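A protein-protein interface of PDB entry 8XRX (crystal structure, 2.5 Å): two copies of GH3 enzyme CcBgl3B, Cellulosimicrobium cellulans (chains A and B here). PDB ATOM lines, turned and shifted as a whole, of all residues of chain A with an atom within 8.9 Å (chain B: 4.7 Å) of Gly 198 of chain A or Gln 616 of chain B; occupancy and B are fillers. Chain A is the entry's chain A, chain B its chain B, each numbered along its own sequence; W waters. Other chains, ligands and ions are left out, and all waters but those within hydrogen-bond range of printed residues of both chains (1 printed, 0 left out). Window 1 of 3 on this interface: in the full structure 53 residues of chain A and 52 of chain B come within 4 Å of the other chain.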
ATOM      1  N   ASP A 144     -18.700   7.226  -9.015  1.00  0.00           N
ATOM      2  CA  ASP A 144     -18.655   8.655  -8.725  1.00  0.00           C
ATOM      3  C   ASP A 144     -18.012   8.821  -7.358  1.00  0.00           C
ATOM      4  O   ASP A 144     -18.550   8.333  -6.364  1.00  0.00           O
ATOM      5  CB  ASP A 144     -20.058   9.272  -8.770  1.00  0.00           C
ATOM      6  CG  ASP A 144     -20.044  10.791  -8.713  1.00  0.00           C
ATOM      7  OD1 ASP A 144     -19.188  11.383  -8.032  1.00  0.00           O
ATOM      8  OD2 ASP A 144     -20.904  11.411  -9.361  1.00  0.00           O
ATOM      9  N   LEU A 145     -16.860   9.498  -7.311  1.00  0.00           N
ATOM     10  CA  LEU A 145     -16.090   9.608  -6.071  1.00  0.00           C
ATOM     11  C   LEU A 145     -16.778  10.455  -5.006  1.00  0.00           C
ATOM     12  O   LEU A 145     -16.433  10.332  -3.830  1.00  0.00           O
ATOM     13  CB  LEU A 145     -14.700  10.178  -6.358  1.00  0.00           C
ATOM     14  CG  LEU A 145     -13.783   9.292  -7.201  1.00  0.00           C
ATOM     15  CD1 LEU A 145     -12.433   9.937  -7.367  1.00  0.00           C
ATOM     16  CD2 LEU A 145     -13.655   7.920  -6.576  1.00  0.00           C
ATOM     17  N   ARG A 146     -17.707  11.329  -5.410  1.00  0.00           N
ATOM     18  CA  ARG A 146     -18.508  12.127  -4.494  1.00  0.00           C
ATOM     19  C   ARG A 146     -19.377  11.285  -3.575  1.00  0.00           C
ATOM     20  O   ARG A 146     -19.739  11.749  -2.497  1.00  0.00           O
ATOM     21  CB  ARG A 146     -19.406  13.074  -5.278  1.00  0.00           C
ATOM     22  CG  ARG A 146     -18.664  14.168  -6.036  1.00  0.00           C
ATOM     23  CD  ARG A 146     -19.623  15.066  -6.746  1.00  0.00           C
ATOM     24  NE  ARG A 146     -20.271  14.336  -7.828  1.00  0.00           N
ATOM     25  CZ  ARG A 146     -21.107  14.868  -8.705  1.00  0.00           C
ATOM     26  NH1 ARG A 146     -21.639  14.113  -9.626  1.00  0.00           N
ATOM     27  NH2 ARG A 146     -21.415  16.143  -8.648  1.00  0.00           N
ATOM     28  N   TRP A 147     -19.712  10.066  -3.970  1.00  0.00           N
ATOM     29  CA  TRP A 147     -20.597   9.233  -3.182  1.00  0.00           C
ATOM     30  C   TRP A 147     -20.028   8.970  -1.798  1.00  0.00           C
ATOM     31  O   TRP A 147     -18.841   8.701  -1.631  1.00  0.00           O
ATOM     32  CB  TRP A 147     -20.837   7.923  -3.916  1.00  0.00           C
ATOM     33  CG  TRP A 147     -22.043   7.137  -3.499  1.00  0.00           C
ATOM     34  CD1 TRP A 147     -23.316   7.594  -3.333  1.00  0.00           C
ATOM     35  CD2 TRP A 147     -22.088   5.732  -3.261  1.00  0.00           C
ATOM     36  NE1 TRP A 147     -24.143   6.563  -2.976  1.00  0.00           N
ATOM     37  CE2 TRP A 147     -23.415   5.405  -2.943  1.00  0.00           C
ATOM     38  CE3 TRP A 147     -21.129   4.717  -3.288  1.00  0.00           C
ATOM     39  CZ2 TRP A 147     -23.800   4.124  -2.646  1.00  0.00           C
ATOM     40  CZ3 TRP A 147     -21.516   3.452  -2.999  1.00  0.00           C
ATOM     41  CH2 TRP A 147     -22.838   3.158  -2.688  1.00  0.00           C
ATOM     42  N   GLY A 148     -20.896   9.030  -0.796  1.00  0.00           N
ATOM     43  CA  GLY A 148     -20.442   8.879   0.569  1.00  0.00           C
ATOM     44  C   GLY A 148     -20.033   7.474   0.949  1.00  0.00           C
ATOM     45  O   GLY A 148     -19.357   7.307   1.962  1.00  0.00           O
ATOM     46  N   SER A 194     -24.836   2.870  -6.303  1.00  0.00           N
ATOM     47  CA  SER A 194     -23.593   3.636  -6.276  1.00  0.00           C
ATOM     48  C   SER A 194     -23.517   4.793  -7.268  1.00  0.00           C
ATOM     49  O   SER A 194     -22.719   5.706  -7.041  1.00  0.00           O
ATOM     50  CB  SER A 194     -22.406   2.720  -6.528  1.00  0.00           C
ATOM     51  OG  SER A 194     -22.668   1.848  -7.588  1.00  0.00           O
ATOM     52  N   GLU A 195     -24.271   4.776  -8.371  1.00  0.00           N
ATOM     53  CA  GLU A 195     -24.171   5.842  -9.364  1.00  0.00           C
ATOM     54  C   GLU A 195     -25.517   6.532  -9.559  1.00  0.00           C
ATOM     55  O   GLU A 195     -26.295   6.176 -10.443  1.00  0.00           O
ATOM     56  CB  GLU A 195     -23.627   5.326 -10.692  1.00  0.00           C
ATOM     57  CG  GLU A 195     -23.480   6.472 -11.667  1.00  0.00           C
ATOM     58  CD  GLU A 195     -22.561   6.227 -12.846  1.00  0.00           C
ATOM     59  OE1 GLU A 195     -22.152   7.226 -13.462  1.00  0.00           O
ATOM     60  OE2 GLU A 195     -22.258   5.072 -13.174  1.00  0.00           O
ATOM     61  N   THR A 196     -25.772   7.550  -8.756  1.00  0.00           N
ATOM     62  CA  THR A 196     -26.973   8.359  -8.834  1.00  0.00           C
ATOM     63  C   THR A 196     -26.577   9.816  -9.050  1.00  0.00           C
ATOM     64  O   THR A 196     -25.413  10.181  -8.948  1.00  0.00           O
ATOM     65  CB  THR A 196     -27.834   8.190  -7.569  1.00  0.00           C
ATOM     66  OG1 THR A 196     -27.098   8.604  -6.417  1.00  0.00           O
ATOM     67  CG2 THR A 196     -28.252   6.742  -7.387  1.00  0.00           C
ATOM     68  N   GLN A 197     -27.562  10.647  -9.352  1.00  0.00           N
ATOM     69  CA  GLN A 197     -27.309  12.024  -9.737  1.00  0.00           C
ATOM     70  C   GLN A 197     -26.514  12.757  -8.669  1.00  0.00           C
ATOM     71  O   GLN A 197     -26.797  12.645  -7.475  1.00  0.00           O
ATOM     72  CB  GLN A 197     -28.617  12.768  -9.956  1.00  0.00           C
ATOM     73  CG  GLN A 197     -29.534  12.209 -10.965  1.00  0.00           C
ATOM     74  CD  GLN A 197     -30.704  13.138 -11.231  1.00  0.00           C
ATOM     75  OE1 GLN A 197     -31.146  13.869 -10.349  1.00  0.00           O
ATOM     76  NE2 GLN A 197     -31.201  13.125 -12.462  1.00  0.00           N
ATOM     77  N   GLY A 198     -25.533  13.536  -9.115  1.00  0.00           N
ATOM     78  CA  GLY A 198     -24.733  14.343  -8.223  1.00  0.00           C
ATOM     79  C   GLY A 198     -23.899  13.611  -7.195  1.00  0.00           C
ATOM     80  O   GLY A 198     -23.360  14.235  -6.289  1.00  0.00           O
ATOM     81  N   GLY A 199     -23.791  12.298  -7.319  1.00  0.00           N
ATOM     82  CA  GLY A 199     -23.119  11.520  -6.311  1.00  0.00           C
ATOM     83  C   GLY A 199     -23.847  11.405  -4.999  1.00  0.00           C
ATOM     84  O   GLY A 199     -23.289  10.864  -4.048  1.00  0.00           O
ATOM     85  N   ARG A 200     -25.091  11.862  -4.935  1.00  0.00           N
ATOM     86  CA  ARG A 200     -25.847  11.956  -3.698  1.00  0.00           C
ATOM     87  C   ARG A 200     -26.346  10.581  -3.253  1.00  0.00           C
ATOM     88  O   ARG A 200     -26.224   9.581  -3.958  1.00  0.00           O
ATOM     89  CB  ARG A 200     -26.986  12.940  -3.884  1.00  0.00           C
ATOM     90  CG  ARG A 200     -26.487  14.305  -4.279  1.00  0.00           C
ATOM     91  CD  ARG A 200     -27.493  15.118  -5.040  1.00  0.00           C
ATOM     92  NE  ARG A 200     -26.913  16.382  -5.448  1.00  0.00           N
ATOM     93  CZ  ARG A 200     -27.556  17.378  -6.044  1.00  0.00           C
ATOM     94  NH1 ARG A 200     -28.843  17.291  -6.330  1.00  0.00           N
ATOM     95  NH2 ARG A 200     -26.901  18.483  -6.333  1.00  0.00           N
ATOM     96  N   ASP A 201     -26.880  10.529  -2.037  1.00  0.00           N
ATOM     97  CA  ASP A 201     -27.351   9.273  -1.459  1.00  0.00           C
ATOM     98  C   ASP A 201     -28.798   9.034  -1.886  1.00  0.00           C
ATOM     99  O   ASP A 201     -29.711   9.768  -1.480  1.00  0.00           O
ATOM    100  CB  ASP A 201     -27.215   9.279   0.053  1.00  0.00           C
ATOM    101  CG  ASP A 201     -27.394   7.899   0.665  1.00  0.00           C
ATOM    102  OD1 ASP A 201     -27.483   6.901  -0.064  1.00  0.00           O
ATOM    103  OD2 ASP A 201     -27.412   7.800   1.908  1.00  0.00           O
ATOM    104  N   ALA A 202     -28.987   8.010  -2.718  1.00  0.00           N
ATOM    105  CA  ALA A 202     -30.288   7.551  -3.175  1.00  0.00           C
ATOM    106  C   ALA A 202     -31.061   8.656  -3.870  1.00  0.00           C
ATOM    107  O   ALA A 202     -32.277   8.712  -3.820  1.00  0.00           O
ATOM    108  CB  ALA A 202     -31.105   6.955  -2.035  1.00  0.00           C
ATOM    109  N   SER A 203     -30.362   9.558  -4.519  1.00  0.00           N
ATOM    110  CA  SER A 203     -30.996  10.367  -5.539  1.00  0.00           C
ATOM    111  C   SER A 203     -31.332   9.447  -6.713  1.00  0.00           C
ATOM    112  O   SER A 203     -31.206   8.224  -6.643  1.00  0.00           O
ATOM    113  CB  SER A 203     -30.085  11.517  -5.937  1.00  0.00           C
ATOM    114  OG  SER A 203     -28.848  11.002  -6.354  1.00  0.00           O
ATOM    115  N   GLU A 204     -31.752  10.040  -7.816  1.00  0.00           N
ATOM    116  CA  GLU A 204     -32.200   9.263  -8.960  1.00  0.00           C
ATOM    117  C   GLU A 204     -31.036   8.578  -9.662  1.00  0.00           C
ATOM    118  O   GLU A 204     -30.011   9.197  -9.948  1.00  0.00           O
ATOM    119  CB  GLU A 204     -32.942  10.165  -9.942  1.00  0.00           C
ATOM    120  CG  GLU A 204     -33.444   9.453 -11.170  1.00  0.00           C
ATOM    121  CD  GLU A 204     -34.810   8.816 -10.966  1.00  0.00           C
ATOM    122  OE1 GLU A 204     -35.299   8.191 -11.908  1.00  0.00           O
ATOM    123  OE2 GLU A 204     -35.422   8.933  -9.896  1.00  0.00           O
ATOM    124  N   ALA A 205     -31.202   7.295  -9.940  1.00  0.00           N
ATOM    125  CA  ALA A 205     -30.274   6.562 -10.778  1.00  0.00           C
ATOM    126  C   ALA A 205     -30.751   6.648 -12.231  1.00  0.00           C
ATOM    127  O   ALA A 205     -31.778   6.074 -12.591  1.00  0.00           O
ATOM    128  CB  ALA A 205     -30.163   5.124 -10.305  1.00  0.00           C
ATOM    129  N   ASP A 206     -30.001   7.372 -13.061  1.00  0.00           N
ATOM    130  CA  ASP A 206     -30.338   7.576 -14.469  1.00  0.00           C
ATOM    131  C   ASP A 206     -29.749   6.455 -15.324  1.00  0.00           C
ATOM    132  O   ASP A 206     -28.968   6.671 -16.227  1.00  0.00           O
ATOM    133  CB  ASP A 206     -29.829   8.934 -14.936  1.00  0.00           C
ATOM    134  CG  ASP A 206     -30.727  10.075 -14.515  1.00  0.00           C
ATOM    135  OD1 ASP A 206     -31.951   9.863 -14.389  1.00  0.00           O
ATOM    136  OD2 ASP A 206     -30.213  11.194 -14.338  1.00  0.00           O
ATOM    137  N   SER A 531     -22.554  12.467   1.264  1.00  0.00           N
ATOM    138  CA  SER A 531     -21.768  12.622   0.054  1.00  0.00           C
ATOM    139  C   SER A 531     -20.984  13.926   0.131  1.00  0.00           C
ATOM    140  O   SER A 531     -21.335  14.836   0.876  1.00  0.00           O
ATOM    141  CB  SER A 531     -22.679  12.604  -1.182  1.00  0.00           C
ATOM    142  OG  SER A 531     -23.163  11.304  -1.447  1.00  0.00           O
ATOM    143  N   THR A 532     -19.904  14.011  -0.631  1.00  0.00           N
ATOM    144  CA  THR A 532     -19.066  15.203  -0.639  1.00  0.00           C
ATOM    145  C   THR A 532     -18.982  15.779  -2.043  1.00  0.00           C
ATOM    146  O   THR A 532     -19.017  15.048  -3.023  1.00  0.00           O
ATOM    147  CB  THR A 532     -17.639  14.930  -0.110  1.00  0.00           C
ATOM    148  OG1 THR A 532     -17.035  13.837  -0.816  1.00  0.00           O
ATOM    149  CG2 THR A 532     -17.668  14.624   1.359  1.00  0.00           C
ATOM    150  N   ALA A 533     -18.870  17.097  -2.129  1.00  0.00           N
ATOM    151  CA  ALA A 533     -18.832  17.762  -3.419  1.00  0.00           C
ATOM    152  C   ALA A 533     -17.413  18.048  -3.924  1.00  0.00           C
ATOM    153  O   ALA A 533     -17.158  17.921  -5.117  1.00  0.00           O
ATOM    154  CB  ALA A 533     -19.629  19.066  -3.362  1.00  0.00           C
ATOM    155  N   THR A 534     -16.479  18.458  -3.060  1.00  0.00           N
ATOM    156  CA  THR A 534     -15.181  18.905  -3.534  1.00  0.00           C
ATOM    157  C   THR A 534     -14.107  17.835  -3.503  1.00  0.00           C
ATOM    158  O   THR A 534     -13.129  17.952  -4.251  1.00  0.00           O
ATOM    159  CB  THR A 534     -14.688  20.102  -2.726  1.00  0.00           C
ATOM    160  OG1 THR A 534     -14.276  19.662  -1.434  1.00  0.00           O
ATOM    161  CG2 THR A 534     -15.785  21.102  -2.580  1.00  0.00           C
ATOM    162  N   LEU A 535     -14.258  16.803  -2.685  1.00  0.00           N
ATOM    163  CA  LEU A 535     -13.252  15.765  -2.493  1.00  0.00           C
ATOM    164  C   LEU A 535     -11.960  16.284  -1.868  1.00  0.00           C
ATOM    165  O   LEU A 535     -11.000  15.546  -1.753  1.00  0.00           O
ATOM    166  CB  LEU A 535     -12.913  15.049  -3.807  1.00  0.00           C
ATOM    167  CG  LEU A 535     -14.059  14.553  -4.681  1.00  0.00           C
ATOM    168  CD1 LEU A 535     -13.499  14.056  -5.991  1.00  0.00           C
ATOM    169  CD2 LEU A 535     -14.870  13.467  -3.994  1.00  0.00           C
ATOM    170  N   LYS A 563     -12.244   7.302   1.031  1.00  0.00           N
ATOM    171  CA  LYS A 563     -12.332   7.275  -0.414  1.00  0.00           C
ATOM    172  C   LYS A 563     -11.209   8.131  -0.967  1.00  0.00           C
ATOM    173  O   LYS A 563     -10.628   8.935  -0.241  1.00  0.00           O
ATOM    174  CB  LYS A 563     -13.707   7.776  -0.880  1.00  0.00           C
ATOM    175  CG  LYS A 563     -13.931   9.221  -0.706  1.00  0.00           C
ATOM    176  CD  LYS A 563     -15.397   9.514  -0.691  1.00  0.00           C
ATOM    177  CE  LYS A 563     -15.631  10.965  -0.618  1.00  0.00           C
ATOM    178  NZ  LYS A 563     -17.004  11.262  -0.898  1.00  0.00           N
ATOM    179  N   ALA A 613     -13.087  17.333  -8.719  1.00  0.00           N
ATOM    180  CA  ALA A 613     -14.380  16.663  -8.763  1.00  0.00           C
ATOM    181  C   ALA A 613     -15.013  16.792 -10.143  1.00  0.00           C
ATOM    182  O   ALA A 613     -15.695  15.870 -10.601  1.00  0.00           O
ATOM    183  CB  ALA A 613     -15.308  17.214  -7.679  1.00  0.00           C
ATOM    184  N   GLY A 614     -14.763  17.910 -10.824  1.00  0.00           N
ATOM    185  CA  GLY A 614     -15.236  18.175 -12.167  1.00  0.00           C
ATOM    186  C   GLY A 614     -14.565  17.366 -13.259  1.00  0.00           C
ATOM    187  O   GLY A 614     -15.037  17.392 -14.394  1.00  0.00           O
ATOM    188  N   GLN A 616     -14.407  14.122 -13.432  1.00  0.00           N
ATOM    189  CA  GLN A 616     -15.020  12.807 -13.543  1.00  0.00           C
ATOM    190  C   GLN A 616     -15.893  12.655 -14.789  1.00  0.00           C
ATOM    191  O   GLN A 616     -16.525  13.607 -15.220  1.00  0.00           O
ATOM    192  CB  GLN A 616     -15.847  12.534 -12.299  1.00  0.00           C
ATOM    193  CG  GLN A 616     -15.057  12.453 -11.027  1.00  0.00           C
ATOM    194  CD  GLN A 616     -15.900  11.950  -9.879  1.00  0.00           C
ATOM    195  OE1 GLN A 616     -15.818  10.791  -9.500  1.00  0.00           O
ATOM    196  NE2 GLN A 616     -16.734  12.816  -9.342  1.00  0.00           N
ATOM    197  N   ARG B 143     -27.801  21.053 -18.912  1.00  0.00           N
ATOM    198  CA  ARG B 143     -27.926  20.341 -17.657  1.00  0.00           C
ATOM    199  C   ARG B 143     -26.606  20.136 -16.932  1.00  0.00           C
ATOM    200  O   ARG B 143     -26.628  19.898 -15.723  1.00  0.00           O
ATOM    201  CB  ARG B 143     -28.568  18.979 -17.879  1.00  0.00           C
ATOM    202  CG  ARG B 143     -29.897  19.045 -18.575  1.00  0.00           C
ATOM    203  CD  ARG B 143     -30.680  17.814 -18.299  1.00  0.00           C
ATOM    204  NE  ARG B 143     -31.738  18.118 -17.380  1.00  0.00           N
ATOM    205  CZ  ARG B 143     -32.272  17.253 -16.538  1.00  0.00           C
ATOM    206  NH1 ARG B 143     -31.826  16.007 -16.468  1.00  0.00           N
ATOM    207  NH2 ARG B 143     -33.250  17.670 -15.767  1.00  0.00           N
ATOM    208  N   ASP B 144     -25.475  20.200 -17.635  1.00  0.00           N
ATOM    209  CA  ASP B 144     -24.151  20.126 -17.032  1.00  0.00           C
ATOM    210  C   ASP B 144     -23.354  21.347 -17.459  1.00  0.00           C
ATOM    211  O   ASP B 144     -23.042  21.504 -18.644  1.00  0.00           O
ATOM    212  CB  ASP B 144     -23.423  18.847 -17.437  1.00  0.00           C
ATOM    213  CG  ASP B 144     -22.144  18.622 -16.638  1.00  0.00           C
ATOM    214  OD1 ASP B 144     -21.475  19.594 -16.261  1.00  0.00           O
ATOM    215  OD2 ASP B 144     -21.792  17.466 -16.375  1.00  0.00           O
ATOM    216  N   LEU B 145     -22.999  22.190 -16.491  1.00  0.00           N
ATOM    217  CA  LEU B 145     -22.315  23.438 -16.786  1.00  0.00           C
ATOM    218  C   LEU B 145     -20.909  23.215 -17.308  1.00  0.00           C
ATOM    219  O   LEU B 145     -20.322  24.136 -17.869  1.00  0.00           O
ATOM    220  CB  LEU B 145     -22.277  24.315 -15.534  1.00  0.00           C
ATOM    221  CG  LEU B 145     -23.615  24.791 -14.977  1.00  0.00           C
ATOM    222  CD1 LEU B 145     -23.431  25.660 -13.760  1.00  0.00           C
ATOM    223  CD2 LEU B 145     -24.391  25.527 -16.031  1.00  0.00           C
ATOM    224  N   ARG B 146     -20.352  22.024 -17.121  1.00  0.00           N
ATOM    225  CA  ARG B 146     -19.028  21.737 -17.653  1.00  0.00           C
ATOM    226  C   ARG B 146     -19.009  21.749 -19.176  1.00  0.00           C
ATOM    227  O   ARG B 146     -17.976  22.067 -19.771  1.00  0.00           O
ATOM    228  CB  ARG B 146     -18.529  20.394 -17.119  1.00  0.00           C
ATOM    229  CG  ARG B 146     -18.186  20.427 -15.642  1.00  0.00           C
ATOM    230  CD  ARG B 146     -17.776  19.080 -15.151  1.00  0.00           C
ATOM    231  NE  ARG B 146     -18.830  18.112 -15.333  1.00  0.00           N
ATOM    232  CZ  ARG B 146     -18.699  16.824 -15.069  1.00  0.00           C
ATOM    233  NH1 ARG B 146     -19.720  16.012 -15.240  1.00  0.00           N
ATOM    234  NH2 ARG B 146     -17.544  16.353 -14.631  1.00  0.00           N
ATOM    235  N   ALA B 610     -23.632  27.245 -10.328  1.00  0.00           N
ATOM    236  CA  ALA B 610     -23.141  26.376  -9.275  1.00  0.00           C
ATOM    237  C   ALA B 610     -22.100  27.086  -8.400  1.00  0.00           C
ATOM    238  O   ALA B 610     -21.489  28.085  -8.779  1.00  0.00           O
ATOM    239  CB  ALA B 610     -22.552  25.098  -9.866  1.00  0.00           C
ATOM    240  N   HIS B 612     -19.662  25.132  -7.086  1.00  0.00           N
ATOM    241  CA  HIS B 612     -18.550  24.243  -7.328  1.00  0.00           C
ATOM    242  C   HIS B 612     -19.021  23.252  -8.380  1.00  0.00           C
ATOM    243  O   HIS B 612     -20.206  22.959  -8.465  1.00  0.00           O
ATOM    244  CB  HIS B 612     -18.144  23.549  -6.038  1.00  0.00           C
ATOM    245  CG  HIS B 612     -16.843  22.831  -6.117  1.00  0.00           C
ATOM    246  ND1 HIS B 612     -16.708  21.599  -6.712  1.00  0.00           N
ATOM    247  CD2 HIS B 612     -15.618  23.173  -5.669  1.00  0.00           C
ATOM    248  CE1 HIS B 612     -15.450  21.216  -6.631  1.00  0.00           C
ATOM    249  NE2 HIS B 612     -14.769  22.156  -6.004  1.00  0.00           N
ATOM    250  N   ALA B 613     -18.103  22.760  -9.194  1.00  0.00           N
ATOM    251  CA  ALA B 613     -18.506  21.815 -10.227  1.00  0.00           C
ATOM    252  C   ALA B 613     -19.079  20.541  -9.626  1.00  0.00           C
ATOM    253  O   ALA B 613     -19.986  19.934 -10.213  1.00  0.00           O
ATOM    254  CB  ALA B 613     -17.332  21.480 -11.149  1.00  0.00           C
ATOM    255  N   GLY B 614     -18.570  20.119  -8.465  1.00  0.00           N
ATOM    256  CA  GLY B 614     -19.067  18.927  -7.795  1.00  0.00           C
ATOM    257  C   GLY B 614     -20.416  19.082  -7.119  1.00  0.00           C
ATOM    258  O   GLY B 614     -20.957  18.097  -6.622  1.00  0.00           O
ATOM    259  N   GLN B 615     -20.963  20.295  -7.084  1.00  0.00           N
ATOM    260  CA  GLN B 615     -22.293  20.542  -6.577  1.00  0.00           C
ATOM    261  C   GLN B 615     -23.387  20.076  -7.536  1.00  0.00           C
ATOM    262  O   GLN B 615     -24.516  19.850  -7.106  1.00  0.00           O
ATOM    263  CB  GLN B 615     -22.445  22.035  -6.278  1.00  0.00           C
ATOM    264  CG  GLN B 615     -23.589  22.368  -5.341  1.00  0.00           C
ATOM    265  CD  GLN B 615     -23.858  23.838  -5.255  1.00  0.00           C
ATOM    266  OE1 GLN B 615     -23.751  24.534  -6.242  1.00  0.00           O
ATOM    267  NE2 GLN B 615     -24.207  24.319  -4.087  1.00  0.00           N
ATOM    268  N   GLN B 616     -23.082  19.917  -8.812  1.00  0.00           N
ATOM    269  CA  GLN B 616     -24.079  19.558  -9.814  1.00  0.00           C
ATOM    270  C   GLN B 616     -24.748  18.234  -9.535  1.00  0.00           C
ATOM    271  O   GLN B 616     -24.121  17.324  -9.068  1.00  0.00           O
ATOM    272  CB  GLN B 616     -23.437  19.534 -11.182  1.00  0.00           C
ATOM    273  CG  GLN B 616     -22.939  20.888 -11.616  1.00  0.00           C
ATOM    274  CD  GLN B 616     -22.715  20.959 -13.100  1.00  0.00           C
ATOM    275  OE1 GLN B 616     -23.572  21.432 -13.839  1.00  0.00           O
ATOM    276  NE2 GLN B 616     -21.578  20.455 -13.549  1.00  0.00           N
ATOM    277  N   PRO B 617     -26.023  18.110  -9.874  1.00  0.00           N
ATOM    278  CA  PRO B 617     -26.846  19.034 -10.644  1.00  0.00           C
ATOM    279  C   PRO B 617     -27.351  20.230  -9.872  1.00  0.00           C
ATOM    280  O   PRO B 617     -27.762  20.095  -8.735  1.00  0.00           O
ATOM    281  CB  PRO B 617     -28.020  18.157 -11.080  1.00  0.00           C
ATOM    282  CG  PRO B 617     -28.131  17.172 -10.012  1.00  0.00           C
ATOM    283  CD  PRO B 617     -26.734  16.855  -9.610  1.00  0.00           C
ATOM    284  N   THR B 618     -27.338  21.389 -10.524  1.00  0.00           N
ATOM    285  CA  THR B 618     -27.819  22.619  -9.928  1.00  0.00           C
ATOM    286  C   THR B 618     -28.978  23.239 -10.697  1.00  0.00           C
ATOM    287  O   THR B 618     -29.369  24.365 -10.390  1.00  0.00           O
ATOM    288  CB  THR B 618     -26.667  23.625  -9.797  1.00  0.00           C
ATOM    289  OG1 THR B 618     -25.822  23.530 -10.951  1.00  0.00           O
ATOM    290  CG2 THR B 618     -25.841  23.358  -8.536  1.00  0.00           C
ATOM    291  N   TYR B 631     -24.396  18.259   0.648  1.00  0.00           N
ATOM    292  CA  TYR B 631     -23.151  17.528   0.752  1.00  0.00           C
ATOM    293  C   TYR B 631     -22.502  17.833   2.100  1.00  0.00           C
ATOM    294  O   TYR B 631     -22.676  18.913   2.663  1.00  0.00           O
ATOM    295  CB  TYR B 631     -22.213  17.908  -0.398  1.00  0.00           C
ATOM    296  CG  TYR B 631     -22.700  17.584  -1.790  1.00  0.00           C
ATOM    297  CD1 TYR B 631     -22.498  16.333  -2.330  1.00  0.00           C
ATOM    298  CD2 TYR B 631     -23.333  18.538  -2.571  1.00  0.00           C
ATOM    299  CE1 TYR B 631     -22.910  16.027  -3.594  1.00  0.00           C
ATOM    300  CE2 TYR B 631     -23.764  18.241  -3.832  1.00  0.00           C
ATOM    301  CZ  TYR B 631     -23.544  16.980  -4.349  1.00  0.00           C
ATOM    302  OH  TYR B 631     -23.949  16.652  -5.615  1.00  0.00           O
HETATM  303  O   HOH W   1     -33.354  14.581 -14.134  1.00  0.00           O
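The backbone carbonyl oxygen (O) of Gly 614 of chain B lies within hydrogen-bond range of the guanidinium group (NH2) of Arg 146 of chain A, at 2.9 Å.
The guanidinium group (NH2) of Arg 146 of chain A sits at hydrogen-bond distance from the backbone carbonyl oxygen (O) of Gln 616 of chain B, at 3.0 Å.
The side-chain hydroxyl of Tyr 631 of chain B is in hydrogen-bond range of the backbone carbonyl oxygen of Gly 198 of chain A, 2.6 Å away.
The backbone carbonyl oxygen (O) of Gln 615 of chain B is in hydrogen-bond range of the guanidinium group (NH2) of Arg 200 of chain A (2.9 Å).
NH2 of Arg 200 of chain A sits at hydrogen-bond distance from O of Pro 617 of chain B, 3.0 Å away.
The guanidinium group of Arg 200 of chain A is in hydrogen-bond range of the side-chain hydroxyl of Tyr 631 of chain B (3.0 Å).
NH2 of Arg 146 of chain B is in hydrogen-bond range of O of Gly 614 of chain A (2.7 Å).
O of Gln 616 of chain A lies within hydrogen-bond range of NH2 of Arg 146 of chain B, at 3.0 Å.
Water W1 lies within hydrogen-bond range of the side-chain amide nitrogen of Gln 197 of chain A and the guanidinium group of Arg 143 of chain B.
Of the printed residues of chain B, Arg 146 of chain A touches Gly 614 (2.9 Å), Gln 616 (3.0 Å) and Tyr 631 (3.98 Å).
Printed residues of chain B within 4 Å of Arg 200 of chain A: Gln 615 (2.9 Å), Gln 616 (3.9 Å), Pro 617 (3.0 Å) and Tyr 631 (3.0 Å).
No residue of chain A comes within 4 Å of Asp 144 of chain B.
Of chain A, only Arg 146 and Ala 533 come within 4 Å of Gly 614 of chain B.
Of chain A, only Arg 146 (3.0 Å), Gly 198 (3.2 Å) and Arg 200 (3.9 Å) come within 4 Å of Gln 616 of chain B.
Of the printed residues of chain A, Pro 617 of chain B touches Gly 198 (3.5 Å) and Arg 200 (3.0 Å).
The nearest residue of chain A that does not touch Gln 616 of chain B is Gln 197 of chain A (5.2 Å).
The nearest printed residue of chain A that does not touch His 612 of chain B is Ala 533 of chain A (4.01 Å).
Of the 27 printed residues of chain A, 9 touch a printed residue of chain B.
Hydrophobic or aromatic side chains of chain A that line the printed part of chain B: Ala 533.
Hydrophobic or aromatic side chains of chain B that line the printed part of chain A: His 612, Pro 617 and Tyr 631.
Among the printed residues, no Asp or Glu carboxylate lies within 4 Å of a Lys or Arg side-chain nitrogen of the other chain.
Among the printed residues, pairs that only touch across the chains: Gly 198 of chain A with Gln 616 of chain B, Ser 531 of chain A with Tyr 631 of chain B, Ala 533 of chain A with Gly 614 of chain B, Gly 198 of chain A with Pro 617 of chain B, Thr 532 of chain A with Tyr 631 of chain B, Ala 533 of chain A with Tyr 631 of chain B, Thr 534 of chain A with His 612 of chain B, Arg 200 of chain A with Gln 616 of chain B and Arg 146 of chain A with Tyr 631 of chain B.
The backbone carbonyl oxygen of Gly 199 of chain A lies within hydrogen-bond range of the side-chain hydroxyl of Ser 531 of chain A (2.6 Å).
The backbone carbonyl oxygen (O) of Gly 614 of chain B sits at hydrogen-bond distance from the side-chain hydroxyl (OH) of Tyr 631 of chain B (3.5 Å).
Arg 146 of chain A touches Gln 616 of chain B, and with the chains exchanged Gln 616 of chain A touches Arg 146 of chain B.
Positions printed for both chains: 144, 145, 146, 613, 614 and 616.
Of the 17 pairs that touch across the chains among the printed residues, 4 have their exchanged pair printed and touching as well.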
